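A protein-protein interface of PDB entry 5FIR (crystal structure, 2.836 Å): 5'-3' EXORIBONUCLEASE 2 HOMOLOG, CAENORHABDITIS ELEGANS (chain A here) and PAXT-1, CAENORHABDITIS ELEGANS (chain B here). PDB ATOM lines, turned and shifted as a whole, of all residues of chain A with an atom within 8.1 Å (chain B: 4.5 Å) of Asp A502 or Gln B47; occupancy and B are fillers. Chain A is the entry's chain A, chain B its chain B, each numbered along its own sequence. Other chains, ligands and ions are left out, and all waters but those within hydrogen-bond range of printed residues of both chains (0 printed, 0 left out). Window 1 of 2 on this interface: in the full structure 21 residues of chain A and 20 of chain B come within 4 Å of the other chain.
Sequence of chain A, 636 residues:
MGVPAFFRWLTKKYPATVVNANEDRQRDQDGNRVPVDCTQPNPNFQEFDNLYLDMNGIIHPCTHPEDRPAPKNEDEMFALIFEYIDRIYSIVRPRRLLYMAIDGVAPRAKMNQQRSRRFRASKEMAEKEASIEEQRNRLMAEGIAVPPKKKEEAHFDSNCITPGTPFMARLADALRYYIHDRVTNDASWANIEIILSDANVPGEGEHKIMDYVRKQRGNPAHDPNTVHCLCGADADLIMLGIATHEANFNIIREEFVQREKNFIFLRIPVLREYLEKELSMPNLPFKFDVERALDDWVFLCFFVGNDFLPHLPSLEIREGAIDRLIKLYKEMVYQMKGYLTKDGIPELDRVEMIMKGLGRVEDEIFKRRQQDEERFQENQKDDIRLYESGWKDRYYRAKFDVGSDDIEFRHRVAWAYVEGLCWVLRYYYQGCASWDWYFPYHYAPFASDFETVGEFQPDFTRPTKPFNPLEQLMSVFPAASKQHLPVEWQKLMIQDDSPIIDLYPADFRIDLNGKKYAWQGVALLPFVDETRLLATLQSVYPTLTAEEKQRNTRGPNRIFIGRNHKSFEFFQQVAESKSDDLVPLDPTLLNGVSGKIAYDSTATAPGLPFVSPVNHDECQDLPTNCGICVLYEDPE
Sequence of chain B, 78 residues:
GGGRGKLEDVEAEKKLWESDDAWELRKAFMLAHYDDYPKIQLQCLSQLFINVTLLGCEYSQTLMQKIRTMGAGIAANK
Asp A502 touches just these residues of chain B: Cys B44 (3.5 Å), Gln B47 (3.7 Å), Leu B48 (3.8 Å), Asn B51 (3.6 Å) and Tyr B59 (2.7 Å). Of chain A, only Asp A502 (3.7 Å) and Arg A532 (3.9 Å) come within 4 Å of Gln B47. No residue of chain A comes within 4 Å of Ser B46. Printed residues of chain A within 4 Å of Tyr B59: Ile A501, Asp A502 and Pro A505. Printed residues of chain B within 4 Å of Pro A505: Tyr B59. Of the printed residues of chain A, Asn B51 touches Asp A502 and Pro A526. Of the printed residues of chain B, Pro A526 touches Asn B51 (3.3 Å). The nearest printed residue of chain B that does not touch Pro A505 is Asn B51 (6.1 Å).
Hydrophobic or aromatic side chains of chain B within 4 Å of the printed part of chain A: Leu B48 and Tyr B59. Printed residues of chain A that touch a printed residue of chain B: Pro A499, Ile A501, Asp A502, Pro A505, Pro A526, Asp A529 and Arg A532. Hydrophobic or aromatic side chains of chain A that line the printed part of chain B: Pro A505 and Pro A526. Among the printed residues, no Asp or Glu carboxylate lies within 4 Å of a Lys or Arg side-chain nitrogen of the other chain.
CE2 of Tyr B59 touches O of Ile A501, 3.6 Å away. OD2 of Asp A502 touches CB of Gln B47, at 3.7 Å. Leu B48 touches Asp A502 (CD1 to CA, 3.8 Å). ND2 of Asn B51 touches O of Asp A502, 3.6 Å away. Pro A505 touches Tyr B59 (CA to CE2, 3.7 Å). Pro A526 touches Asn B51 (CG to ND2, 3.3 Å). Arg A532 touches Gln B43. Arg A532 touches Cys B44. Gln B47 touches Arg A532.
The guanidinium group of Arg A115 sits at hydrogen-bond distance from the backbone carbonyl oxygen of Pro A526 (2.8 Å). The side-chain hydroxyl (OG) of Ser A498 is in hydrogen-bond range of the backbone NH (N) of Ile A501 (3.1 Å). O of Arg A532 is in hydrogen-bond range of OG1 of Thr A536 (2.9 Å). The backbone carbonyl oxygen of Gln B43 is in hydrogen-bond range of the side-chain hydroxyl of Ser B46 (3.0 Å). The backbone carbonyl oxygen (O) of Gln B47 sits close to the side-chain amide nitrogen (ND2) of Asn B51 (3.4 Å). ND2 of Asn B51 sits at hydrogen-bond distance from OH of Tyr B59, 2.9 Å away.
The backbone carbonyl oxygen (O) of Pro A499 lies close to the side-chain sulfur (SG) of Cys B44 (3.6 Å). OD1 of Asp A502 is in hydrogen-bond range of SG of Cys B44 (3.5 Å). O of Asp A502 sits at hydrogen-bond distance from OH of Tyr B59 (2.7 Å). The side-chain amide nitrogen of Gln B43 lies within hydrogen-bond range of the side-chain carboxylate of Asp A529.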
ATOM      1  N   ARG A 115       7.923  13.104 -19.583  1.00  0.00           N
ATOM      2  CA  ARG A 115       8.836  14.141 -19.101  1.00  0.00           C
ATOM      3  C   ARG A 115      10.123  13.537 -18.556  1.00  0.00           C
ATOM      4  O   ARG A 115      11.230  13.956 -18.920  1.00  0.00           O
ATOM      5  CB  ARG A 115       8.158  14.942 -18.003  1.00  0.00           C
ATOM      6  CG  ARG A 115       9.035  15.961 -17.289  1.00  0.00           C
ATOM      7  CD  ARG A 115       8.194  16.705 -16.239  1.00  0.00           C
ATOM      8  NE  ARG A 115       8.460  18.141 -16.193  1.00  0.00           N
ATOM      9  CZ  ARG A 115       9.216  18.732 -15.291  1.00  0.00           C
ATOM     10  NH1 ARG A 115       9.769  18.009 -14.340  1.00  0.00           N
ATOM     11  NH2 ARG A 115       9.390  20.042 -15.323  1.00  0.00           N
ATOM     12  N   PHE A 119      13.767  14.471 -20.244  1.00  0.00           N
ATOM     13  CA  PHE A 119      14.769  15.061 -19.360  1.00  0.00           C
ATOM     14  C   PHE A 119      15.979  14.150 -19.232  1.00  0.00           C
ATOM     15  O   PHE A 119      17.134  14.610 -19.267  1.00  0.00           O
ATOM     16  CB  PHE A 119      14.154  15.319 -17.995  1.00  0.00           C
ATOM     17  CG  PHE A 119      13.617  16.689 -17.833  1.00  0.00           C
ATOM     18  CD1 PHE A 119      12.438  17.051 -18.447  1.00  0.00           C
ATOM     19  CD2 PHE A 119      14.253  17.591 -17.019  1.00  0.00           C
ATOM     20  CE1 PHE A 119      11.940  18.296 -18.303  1.00  0.00           C
ATOM     21  CE2 PHE A 119      13.751  18.840 -16.861  1.00  0.00           C
ATOM     22  CZ  PHE A 119      12.583  19.195 -17.501  1.00  0.00           C
ATOM     23  N   LEU A 492      10.487  31.369 -21.501  1.00  0.00           N
ATOM     24  CA  LEU A 492       9.902  30.867 -20.267  1.00  0.00           C
ATOM     25  C   LEU A 492      10.646  29.647 -19.710  1.00  0.00           C
ATOM     26  O   LEU A 492      10.471  29.321 -18.527  1.00  0.00           O
ATOM     27  CB  LEU A 492       8.427  30.551 -20.492  1.00  0.00           C
ATOM     28  CG  LEU A 492       7.417  31.661 -20.224  1.00  0.00           C
ATOM     29  CD1 LEU A 492       7.863  33.046 -20.697  1.00  0.00           C
ATOM     30  CD2 LEU A 492       6.140  31.243 -20.918  1.00  0.00           C
ATOM     31  N   MET A 493      11.484  28.985 -20.514  1.00  0.00           N
ATOM     32  CA  MET A 493      12.189  27.786 -20.052  1.00  0.00           C
ATOM     33  C   MET A 493      13.608  28.057 -19.505  1.00  0.00           C
ATOM     34  O   MET A 493      14.200  27.203 -18.836  1.00  0.00           O
ATOM     35  CB  MET A 493      12.284  26.746 -21.179  1.00  0.00           C
ATOM     36  CG  MET A 493      10.978  26.438 -21.926  1.00  0.00           C
ATOM     37  SD  MET A 493      11.228  25.266 -23.516  1.00  0.00           S
ATOM     38  CE  MET A 493      10.803  23.549 -22.717  1.00  0.00           C
ATOM     39  N   ILE A 494      14.173  29.232 -19.771  1.00  0.00           N
ATOM     40  CA  ILE A 494      15.588  29.404 -19.468  1.00  0.00           C
ATOM     41  C   ILE A 494      15.903  30.632 -18.614  1.00  0.00           C
ATOM     42  O   ILE A 494      16.812  30.589 -17.773  1.00  0.00           O
ATOM     43  CB  ILE A 494      16.409  29.444 -20.768  1.00  0.00           C
ATOM     44  CG1 ILE A 494      16.105  30.701 -21.571  1.00  0.00           C
ATOM     45  CG2 ILE A 494      16.135  28.221 -21.622  1.00  0.00           C
ATOM     46  CD1 ILE A 494      17.014  30.863 -22.763  1.00  0.00           C
ATOM     47  N   GLN A 495      15.168  31.729 -18.783  1.00  0.00           N
ATOM     48  CA  GLN A 495      15.606  32.936 -18.102  1.00  0.00           C
ATOM     49  C   GLN A 495      15.127  32.969 -16.658  1.00  0.00           C
ATOM     50  O   GLN A 495      14.102  32.394 -16.302  1.00  0.00           O
ATOM     51  CB  GLN A 495      15.167  34.203 -18.840  1.00  0.00           C
ATOM     52  CG  GLN A 495      13.726  34.351 -19.218  1.00  0.00           C
ATOM     53  CD  GLN A 495      13.540  35.459 -20.264  1.00  0.00           C
ATOM     54  OE1 GLN A 495      14.363  35.637 -21.175  1.00  0.00           O
ATOM     55  NE2 GLN A 495      12.462  36.220 -20.121  1.00  0.00           N
ATOM     56  N   ASP A 496      15.918  33.623 -15.811  1.00  0.00           N
ATOM     57  CA  ASP A 496      15.650  33.542 -14.383  1.00  0.00           C
ATOM     58  C   ASP A 496      14.379  34.281 -14.000  1.00  0.00           C
ATOM     59  O   ASP A 496      13.711  33.900 -13.033  1.00  0.00           O
ATOM     60  CB  ASP A 496      16.877  34.028 -13.620  1.00  0.00           C
ATOM     61  CG  ASP A 496      18.138  33.322 -14.081  1.00  0.00           C
ATOM     62  OD1 ASP A 496      17.995  32.392 -14.914  1.00  0.00           O
ATOM     63  OD2 ASP A 496      19.253  33.687 -13.644  1.00  0.00           O
ATOM     64  N   SER A 498      11.646  34.069 -15.479  1.00  0.00           N
ATOM     65  CA  SER A 498      10.491  33.272 -15.901  1.00  0.00           C
ATOM     66  C   SER A 498       9.768  32.667 -14.705  1.00  0.00           C
ATOM     67  O   SER A 498      10.394  31.976 -13.897  1.00  0.00           O
ATOM     68  CB  SER A 498      10.954  32.148 -16.826  1.00  0.00           C
ATOM     69  OG  SER A 498      10.122  31.003 -16.716  1.00  0.00           O
ATOM     70  N   PRO A 499       8.447  32.824 -14.600  1.00  0.00           N
ATOM     71  CA  PRO A 499       7.717  32.289 -13.444  1.00  0.00           C
ATOM     72  C   PRO A 499       7.465  30.796 -13.496  1.00  0.00           C
ATOM     73  O   PRO A 499       6.748  30.284 -12.626  1.00  0.00           O
ATOM     74  CB  PRO A 499       6.386  33.043 -13.496  1.00  0.00           C
ATOM     75  CG  PRO A 499       6.205  33.374 -14.951  1.00  0.00           C
ATOM     76  CD  PRO A 499       7.572  33.547 -15.539  1.00  0.00           C
ATOM     77  N   ILE A 500       8.043  30.102 -14.482  1.00  0.00           N
ATOM     78  CA  ILE A 500       8.022  28.647 -14.471  1.00  0.00           C
ATOM     79  C   ILE A 500       9.436  28.103 -14.629  1.00  0.00           C
ATOM     80  O   ILE A 500       9.611  26.916 -14.910  1.00  0.00           O
ATOM     81  CB  ILE A 500       7.097  28.071 -15.550  1.00  0.00           C
ATOM     82  CG1 ILE A 500       7.488  28.553 -16.940  1.00  0.00           C
ATOM     83  CG2 ILE A 500       5.688  28.473 -15.295  1.00  0.00           C
ATOM     84  CD1 ILE A 500       6.663  27.850 -18.019  1.00  0.00           C
ATOM     85  N   ILE A 501      10.456  28.938 -14.396  1.00  0.00           N
ATOM     86  CA  ILE A 501      11.827  28.459 -14.538  1.00  0.00           C
ATOM     87  C   ILE A 501      12.098  27.262 -13.638  1.00  0.00           C
ATOM     88  O   ILE A 501      13.041  26.502 -13.885  1.00  0.00           O
ATOM     89  CB  ILE A 501      12.841  29.584 -14.267  1.00  0.00           C
ATOM     90  CG1 ILE A 501      14.236  29.122 -14.659  1.00  0.00           C
ATOM     91  CG2 ILE A 501      12.887  29.917 -12.795  1.00  0.00           C
ATOM     92  CD1 ILE A 501      14.346  28.657 -16.061  1.00  0.00           C
ATOM     93  N   ASP A 502      11.317  27.095 -12.568  1.00  0.00           N
ATOM     94  CA  ASP A 502      11.518  25.961 -11.680  1.00  0.00           C
ATOM     95  C   ASP A 502      11.176  24.627 -12.328  1.00  0.00           C
ATOM     96  O   ASP A 502      11.646  23.586 -11.855  1.00  0.00           O
ATOM     97  CB  ASP A 502      10.662  26.107 -10.441  1.00  0.00           C
ATOM     98  CG  ASP A 502       9.196  26.009 -10.747  1.00  0.00           C
ATOM     99  OD1 ASP A 502       8.665  26.943 -11.387  1.00  0.00           O
ATOM    100  OD2 ASP A 502       8.588  24.985 -10.351  1.00  0.00           O
ATOM    101  N   LEU A 503      10.379  24.630 -13.393  1.00  0.00           N
ATOM    102  CA  LEU A 503       9.989  23.386 -14.038  1.00  0.00           C
ATOM    103  C   LEU A 503      11.072  22.853 -14.950  1.00  0.00           C
ATOM    104  O   LEU A 503      10.891  21.780 -15.528  1.00  0.00           O
ATOM    105  CB  LEU A 503       8.725  23.559 -14.885  1.00  0.00           C
ATOM    106  CG  LEU A 503       7.434  24.225 -14.380  1.00  0.00           C
ATOM    107  CD1 LEU A 503       6.391  24.096 -15.501  1.00  0.00           C
ATOM    108  CD2 LEU A 503       6.899  23.786 -12.998  1.00  0.00           C
ATOM    109  N   TYR A 504      12.158  23.596 -15.155  1.00  0.00           N
ATOM    110  CA  TYR A 504      13.204  23.220 -16.104  1.00  0.00           C
ATOM    111  C   TYR A 504      14.560  23.251 -15.408  1.00  0.00           C
ATOM    112  O   TYR A 504      15.398  24.139 -15.650  1.00  0.00           O
ATOM    113  CB  TYR A 504      13.158  24.117 -17.341  1.00  0.00           C
ATOM    114  CG  TYR A 504      11.762  24.179 -17.909  1.00  0.00           C
ATOM    115  CD1 TYR A 504      11.303  23.205 -18.779  1.00  0.00           C
ATOM    116  CD2 TYR A 504      10.887  25.183 -17.539  1.00  0.00           C
ATOM    117  CE1 TYR A 504      10.026  23.257 -19.298  1.00  0.00           C
ATOM    118  CE2 TYR A 504       9.610  25.232 -18.027  1.00  0.00           C
ATOM    119  CZ  TYR A 504       9.183  24.271 -18.911  1.00  0.00           C
ATOM    120  OH  TYR A 504       7.901  24.311 -19.420  1.00  0.00           O
ATOM    121  N   PRO A 505      14.805  22.287 -14.527  1.00  0.00           N
ATOM    122  CA  PRO A 505      16.127  22.191 -13.901  1.00  0.00           C
ATOM    123  C   PRO A 505      17.191  21.775 -14.908  1.00  0.00           C
ATOM    124  O   PRO A 505      16.974  20.921 -15.771  1.00  0.00           O
ATOM    125  CB  PRO A 505      15.936  21.126 -12.810  1.00  0.00           C
ATOM    126  CG  PRO A 505      14.737  20.334 -13.242  1.00  0.00           C
ATOM    127  CD  PRO A 505      13.875  21.243 -14.066  1.00  0.00           C
ATOM    128  N   ALA A 506      18.369  22.378 -14.751  1.00  0.00           N
ATOM    129  CA  ALA A 506      19.519  22.071 -15.595  1.00  0.00           C
ATOM    130  C   ALA A 506      20.032  20.661 -15.345  1.00  0.00           C
ATOM    131  O   ALA A 506      20.462  19.981 -16.286  1.00  0.00           O
ATOM    132  CB  ALA A 506      20.626  23.094 -15.322  1.00  0.00           C
ATOM    133  N   LEU A 525      12.408  14.515 -10.492  1.00  0.00           N
ATOM    134  CA  LEU A 525      12.010  15.747 -11.161  1.00  0.00           C
ATOM    135  C   LEU A 525      10.743  16.308 -10.539  1.00  0.00           C
ATOM    136  O   LEU A 525       9.864  15.535 -10.153  1.00  0.00           O
ATOM    137  CB  LEU A 525      11.766  15.495 -12.646  1.00  0.00           C
ATOM    138  CG  LEU A 525      13.037  15.171 -13.418  1.00  0.00           C
ATOM    139  CD1 LEU A 525      12.719  14.635 -14.787  1.00  0.00           C
ATOM    140  CD2 LEU A 525      13.918  16.414 -13.511  1.00  0.00           C
ATOM    141  N   PRO A 526      10.597  17.627 -10.426  1.00  0.00           N
ATOM    142  CA  PRO A 526       9.360  18.165  -9.845  1.00  0.00           C
ATOM    143  C   PRO A 526       8.172  17.952 -10.786  1.00  0.00           C
ATOM    144  O   PRO A 526       8.295  18.057 -12.007  1.00  0.00           O
ATOM    145  CB  PRO A 526       9.671  19.659  -9.660  1.00  0.00           C
ATOM    146  CG  PRO A 526      10.629  19.949 -10.742  1.00  0.00           C
ATOM    147  CD  PRO A 526      11.456  18.695 -10.960  1.00  0.00           C
ATOM    148  N   PHE A 527       7.016  17.645 -10.206  1.00  0.00           N
ATOM    149  CA  PHE A 527       5.797  17.508 -10.983  1.00  0.00           C
ATOM    150  C   PHE A 527       5.373  18.864 -11.541  1.00  0.00           C
ATOM    151  O   PHE A 527       5.588  19.907 -10.916  1.00  0.00           O
ATOM    152  CB  PHE A 527       4.680  16.922 -10.119  1.00  0.00           C
ATOM    153  CG  PHE A 527       4.901  15.488  -9.764  1.00  0.00           C
ATOM    154  CD1 PHE A 527       4.608  14.488 -10.670  1.00  0.00           C
ATOM    155  CD2 PHE A 527       5.400  15.136  -8.523  1.00  0.00           C
ATOM    156  CE1 PHE A 527       4.824  13.170 -10.353  1.00  0.00           C
ATOM    157  CE2 PHE A 527       5.616  13.811  -8.197  1.00  0.00           C
ATOM    158  CZ  PHE A 527       5.329  12.830  -9.105  1.00  0.00           C
ATOM    159  N   VAL A 528       4.770  18.859 -12.736  1.00  0.00           N
ATOM    160  CA  VAL A 528       4.406  20.132 -13.349  1.00  0.00           C
ATOM    161  C   VAL A 528       3.158  20.705 -12.700  1.00  0.00           C
ATOM    162  O   VAL A 528       2.123  20.034 -12.619  1.00  0.00           O
ATOM    163  CB  VAL A 528       4.177  19.988 -14.846  1.00  0.00           C
ATOM    164  CG1 VAL A 528       3.621  21.309 -15.340  1.00  0.00           C
ATOM    165  CG2 VAL A 528       5.464  19.598 -15.505  1.00  0.00           C
ATOM    166  N   ASP A 529       3.235  21.971 -12.289  1.00  0.00           N
ATOM    167  CA  ASP A 529       2.067  22.698 -11.811  1.00  0.00           C
ATOM    168  C   ASP A 529       1.269  23.053 -13.051  1.00  0.00           C
ATOM    169  O   ASP A 529       1.487  24.078 -13.687  1.00  0.00           O
ATOM    170  CB  ASP A 529       2.467  23.934 -11.018  1.00  0.00           C
ATOM    171  CG  ASP A 529       1.312  24.517 -10.198  1.00  0.00           C
ATOM    172  OD1 ASP A 529       0.148  24.115 -10.435  1.00  0.00           O
ATOM    173  OD2 ASP A 529       1.583  25.365  -9.302  1.00  0.00           O
ATOM    174  N   ARG A 532      -0.312  26.622 -12.911  1.00  0.00           N
ATOM    175  CA  ARG A 532       0.672  27.693 -13.067  1.00  0.00           C
ATOM    176  C   ARG A 532       1.281  27.713 -14.471  1.00  0.00           C
ATOM    177  O   ARG A 532       1.672  28.782 -14.963  1.00  0.00           O
ATOM    178  CB  ARG A 532       1.750  27.573 -11.992  1.00  0.00           C
ATOM    179  CG  ARG A 532       2.913  28.546 -12.155  1.00  0.00           C
ATOM    180  CD  ARG A 532       3.615  28.822 -10.850  1.00  0.00           C
ATOM    181  NE  ARG A 532       4.015  27.599 -10.169  1.00  0.00           N
ATOM    182  CZ  ARG A 532       5.177  26.999 -10.361  1.00  0.00           C
ATOM    183  NH1 ARG A 532       6.047  27.525 -11.223  1.00  0.00           N
ATOM    184  NH2 ARG A 532       5.463  25.892  -9.678  1.00  0.00           N
ATOM    185  N   THR A 536       0.943  30.924 -16.949  1.00  0.00           N
ATOM    186  CA  THR A 536       2.085  31.644 -17.512  1.00  0.00           C
ATOM    187  C   THR A 536       1.965  31.786 -19.019  1.00  0.00           C
ATOM    188  O   THR A 536       2.310  32.833 -19.584  1.00  0.00           O
ATOM    189  CB  THR A 536       3.386  30.925 -17.159  1.00  0.00           C
ATOM    190  OG1 THR A 536       3.518  30.848 -15.739  1.00  0.00           O
ATOM    191  CG2 THR A 536       4.585  31.671 -17.731  1.00  0.00           C
ATOM    192  N   GLU B  18       1.808  16.182  -0.721  1.00  0.00           N
ATOM    193  CA  GLU B  18       3.007  16.750  -0.115  1.00  0.00           C
ATOM    194  C   GLU B  18       3.162  16.148   1.280  1.00  0.00           C
ATOM    195  O   GLU B  18       2.199  16.091   2.054  1.00  0.00           O
ATOM    196  CB  GLU B  18       2.895  18.284  -0.053  1.00  0.00           C
ATOM    197  CG  GLU B  18       4.195  19.075  -0.328  1.00  0.00           C
ATOM    198  CD  GLU B  18       3.971  20.524  -0.820  1.00  0.00           C
ATOM    199  OE1 GLU B  18       2.814  20.906  -1.119  1.00  0.00           O
ATOM    200  OE2 GLU B  18       4.967  21.284  -0.925  1.00  0.00           O
ATOM    201  N   ARG B  26       8.095  24.119   2.779  1.00  0.00           N
ATOM    202  CA  ARG B  26       7.490  25.026   1.808  1.00  0.00           C
ATOM    203  C   ARG B  26       6.700  26.130   2.501  1.00  0.00           C
ATOM    204  O   ARG B  26       6.747  27.290   2.076  1.00  0.00           O
ATOM    205  CB  ARG B  26       6.593  24.255   0.835  1.00  0.00           C
ATOM    206  CG  ARG B  26       7.252  23.892  -0.479  1.00  0.00           C
ATOM    207  CD  ARG B  26       6.417  24.316  -1.662  1.00  0.00           C
ATOM    208  NE  ARG B  26       5.038  23.842  -1.618  1.00  0.00           N
ATOM    209  CZ  ARG B  26       4.050  24.422  -2.296  1.00  0.00           C
ATOM    210  NH1 ARG B  26       4.320  25.474  -3.068  1.00  0.00           N
ATOM    211  NH2 ARG B  26       2.802  23.954  -2.213  1.00  0.00           N
ATOM    212  N   GLN B  43       5.088  31.164  -5.573  1.00  0.00           N
ATOM    213  CA  GLN B  43       4.929  29.758  -5.915  1.00  0.00           C
ATOM    214  C   GLN B  43       6.165  29.223  -6.608  1.00  0.00           C
ATOM    215  O   GLN B  43       6.692  28.162  -6.249  1.00  0.00           O
ATOM    216  CB  GLN B  43       3.736  29.578  -6.837  1.00  0.00           C
ATOM    217  CG  GLN B  43       2.420  29.742  -6.198  1.00  0.00           C
ATOM    218  CD  GLN B  43       1.331  29.400  -7.153  1.00  0.00           C
ATOM    219  OE1 GLN B  43       0.522  30.251  -7.499  1.00  0.00           O
ATOM    220  NE2 GLN B  43       1.297  28.143  -7.600  1.00  0.00           N
ATOM    221  N   CYS B  44       6.640  29.960  -7.612  1.00  0.00           N
ATOM    222  CA  CYS B  44       7.788  29.506  -8.375  1.00  0.00           C
ATOM    223  C   CYS B  44       8.992  29.413  -7.468  1.00  0.00           C
ATOM    224  O   CYS B  44       9.629  28.360  -7.358  1.00  0.00           O
ATOM    225  CB  CYS B  44       8.050  30.457  -9.527  1.00  0.00           C
ATOM    226  SG  CYS B  44       9.580  30.110 -10.367  1.00  0.00           S
ATOM    227  N   LEU B  45       9.295  30.512  -6.782  1.00  0.00           N
ATOM    228  CA  LEU B  45      10.463  30.559  -5.921  1.00  0.00           C
ATOM    229  C   LEU B  45      10.358  29.544  -4.797  1.00  0.00           C
ATOM    230  O   LEU B  45      11.353  28.915  -4.428  1.00  0.00           O
ATOM    231  CB  LEU B  45      10.613  31.961  -5.367  1.00  0.00           C
ATOM    232  CG  LEU B  45      10.923  32.957  -6.460  1.00  0.00           C
ATOM    233  CD1 LEU B  45      10.576  34.354  -6.008  1.00  0.00           C
ATOM    234  CD2 LEU B  45      12.389  32.843  -6.757  1.00  0.00           C
ATOM    235  N   SER B  46       9.156  29.326  -4.268  1.00  0.00           N
ATOM    236  CA  SER B  46       9.050  28.356  -3.190  1.00  0.00           C
ATOM    237  C   SER B  46       9.308  26.953  -3.708  1.00  0.00           C
ATOM    238  O   SER B  46       9.999  26.153  -3.060  1.00  0.00           O
ATOM    239  CB  SER B  46       7.677  28.426  -2.527  1.00  0.00           C
ATOM    240  OG  SER B  46       6.668  27.786  -3.278  1.00  0.00           O
ATOM    241  N   GLN B  47       8.772  26.641  -4.887  1.00  0.00           N
ATOM    242  CA  GLN B  47       9.051  25.342  -5.481  1.00  0.00           C
ATOM    243  C   GLN B  47      10.517  25.211  -5.853  1.00  0.00           C
ATOM    244  O   GLN B  47      11.116  24.137  -5.719  1.00  0.00           O
ATOM    245  CB  GLN B  47       8.150  25.120  -6.679  1.00  0.00           C
ATOM    246  CG  GLN B  47       6.848  24.559  -6.254  1.00  0.00           C
ATOM    247  CD  GLN B  47       7.040  23.177  -5.708  1.00  0.00           C
ATOM    248  OE1 GLN B  47       6.524  22.842  -4.644  1.00  0.00           O
ATOM    249  NE2 GLN B  47       7.837  22.374  -6.408  1.00  0.00           N
ATOM    250  N   LEU B  48      11.109  26.302  -6.304  1.00  0.00           N
ATOM    251  CA  LEU B  48      12.520  26.289  -6.631  1.00  0.00           C
ATOM    252  C   LEU B  48      13.342  25.924  -5.404  1.00  0.00           C
ATOM    253  O   LEU B  48      14.243  25.079  -5.468  1.00  0.00           O
ATOM    254  CB  LEU B  48      12.860  27.666  -7.176  1.00  0.00           C
ATOM    255  CG  LEU B  48      14.085  27.993  -7.975  1.00  0.00           C
ATOM    256  CD1 LEU B  48      14.124  27.097  -9.169  1.00  0.00           C
ATOM    257  CD2 LEU B  48      13.815  29.385  -8.431  1.00  0.00           C
ATOM    258  N   PHE B  49      12.977  26.489  -4.253  1.00  0.00           N
ATOM    259  CA  PHE B  49      13.687  26.222  -3.007  1.00  0.00           C
ATOM    260  C   PHE B  49      13.635  24.748  -2.651  1.00  0.00           C
ATOM    261  O   PHE B  49      14.672  24.108  -2.484  1.00  0.00           O
ATOM    262  CB  PHE B  49      13.090  27.077  -1.891  1.00  0.00           C
ATOM    263  CG  PHE B  49      13.562  26.720  -0.511  1.00  0.00           C
ATOM    264  CD1 PHE B  49      14.916  26.798  -0.179  1.00  0.00           C
ATOM    265  CD2 PHE B  49      12.652  26.401   0.484  1.00  0.00           C
ATOM    266  CE1 PHE B  49      15.362  26.508   1.102  1.00  0.00           C
ATOM    267  CE2 PHE B  49      13.083  26.113   1.767  1.00  0.00           C
ATOM    268  CZ  PHE B  49      14.443  26.168   2.078  1.00  0.00           C
ATOM    269  N   ILE B  50      12.436  24.167  -2.581  1.00  0.00           N
ATOM    270  CA  ILE B  50      12.408  22.770  -2.169  1.00  0.00           C
ATOM    271  C   ILE B  50      12.844  21.838  -3.278  1.00  0.00           C
ATOM    272  O   ILE B  50      13.140  20.674  -3.008  1.00  0.00           O
ATOM    273  CB  ILE B  50      11.056  22.295  -1.627  1.00  0.00           C
ATOM    274  CG1 ILE B  50      10.020  22.318  -2.683  1.00  0.00           C
ATOM    275  CG2 ILE B  50      10.594  23.114  -0.450  1.00  0.00           C
ATOM    276  CD1 ILE B  50       8.905  21.485  -2.222  1.00  0.00           C
ATOM    277  N   ASN B  51      12.874  22.283  -4.527  1.00  0.00           N
ATOM    278  CA  ASN B  51      13.474  21.399  -5.516  1.00  0.00           C
ATOM    279  C   ASN B  51      14.966  21.254  -5.293  1.00  0.00           C
ATOM    280  O   ASN B  51      15.517  20.167  -5.509  1.00  0.00           O
ATOM    281  CB  ASN B  51      13.214  21.897  -6.934  1.00  0.00           C
ATOM    282  CG  ASN B  51      11.814  21.633  -7.378  1.00  0.00           C
ATOM    283  OD1 ASN B  51      11.080  20.887  -6.718  1.00  0.00           O
ATOM    284  ND2 ASN B  51      11.420  22.232  -8.502  1.00  0.00           N
ATOM    285  N   TYR B  59      19.902  24.574 -10.785  1.00  0.00           N
ATOM    286  CA  TYR B  59      19.378  25.606 -11.663  1.00  0.00           C
ATOM    287  C   TYR B  59      20.494  26.540 -12.106  1.00  0.00           C
ATOM    288  O   TYR B  59      21.667  26.190 -12.000  1.00  0.00           O
ATOM    289  CB  TYR B  59      18.240  26.367 -10.974  1.00  0.00           C
ATOM    290  CG  TYR B  59      17.030  25.501 -10.706  1.00  0.00           C
ATOM    291  CD1 TYR B  59      16.924  24.736  -9.552  1.00  0.00           C
ATOM    292  CD2 TYR B  59      16.005  25.420 -11.640  1.00  0.00           C
ATOM    293  CE1 TYR B  59      15.808  23.947  -9.328  1.00  0.00           C
ATOM    294  CE2 TYR B  59      14.891  24.632 -11.436  1.00  0.00           C
ATOM    295  CZ  TYR B  59      14.797  23.903 -10.279  1.00  0.00           C
ATOM    296  OH  TYR B  59      13.675  23.134 -10.093  1.00  0.00           O
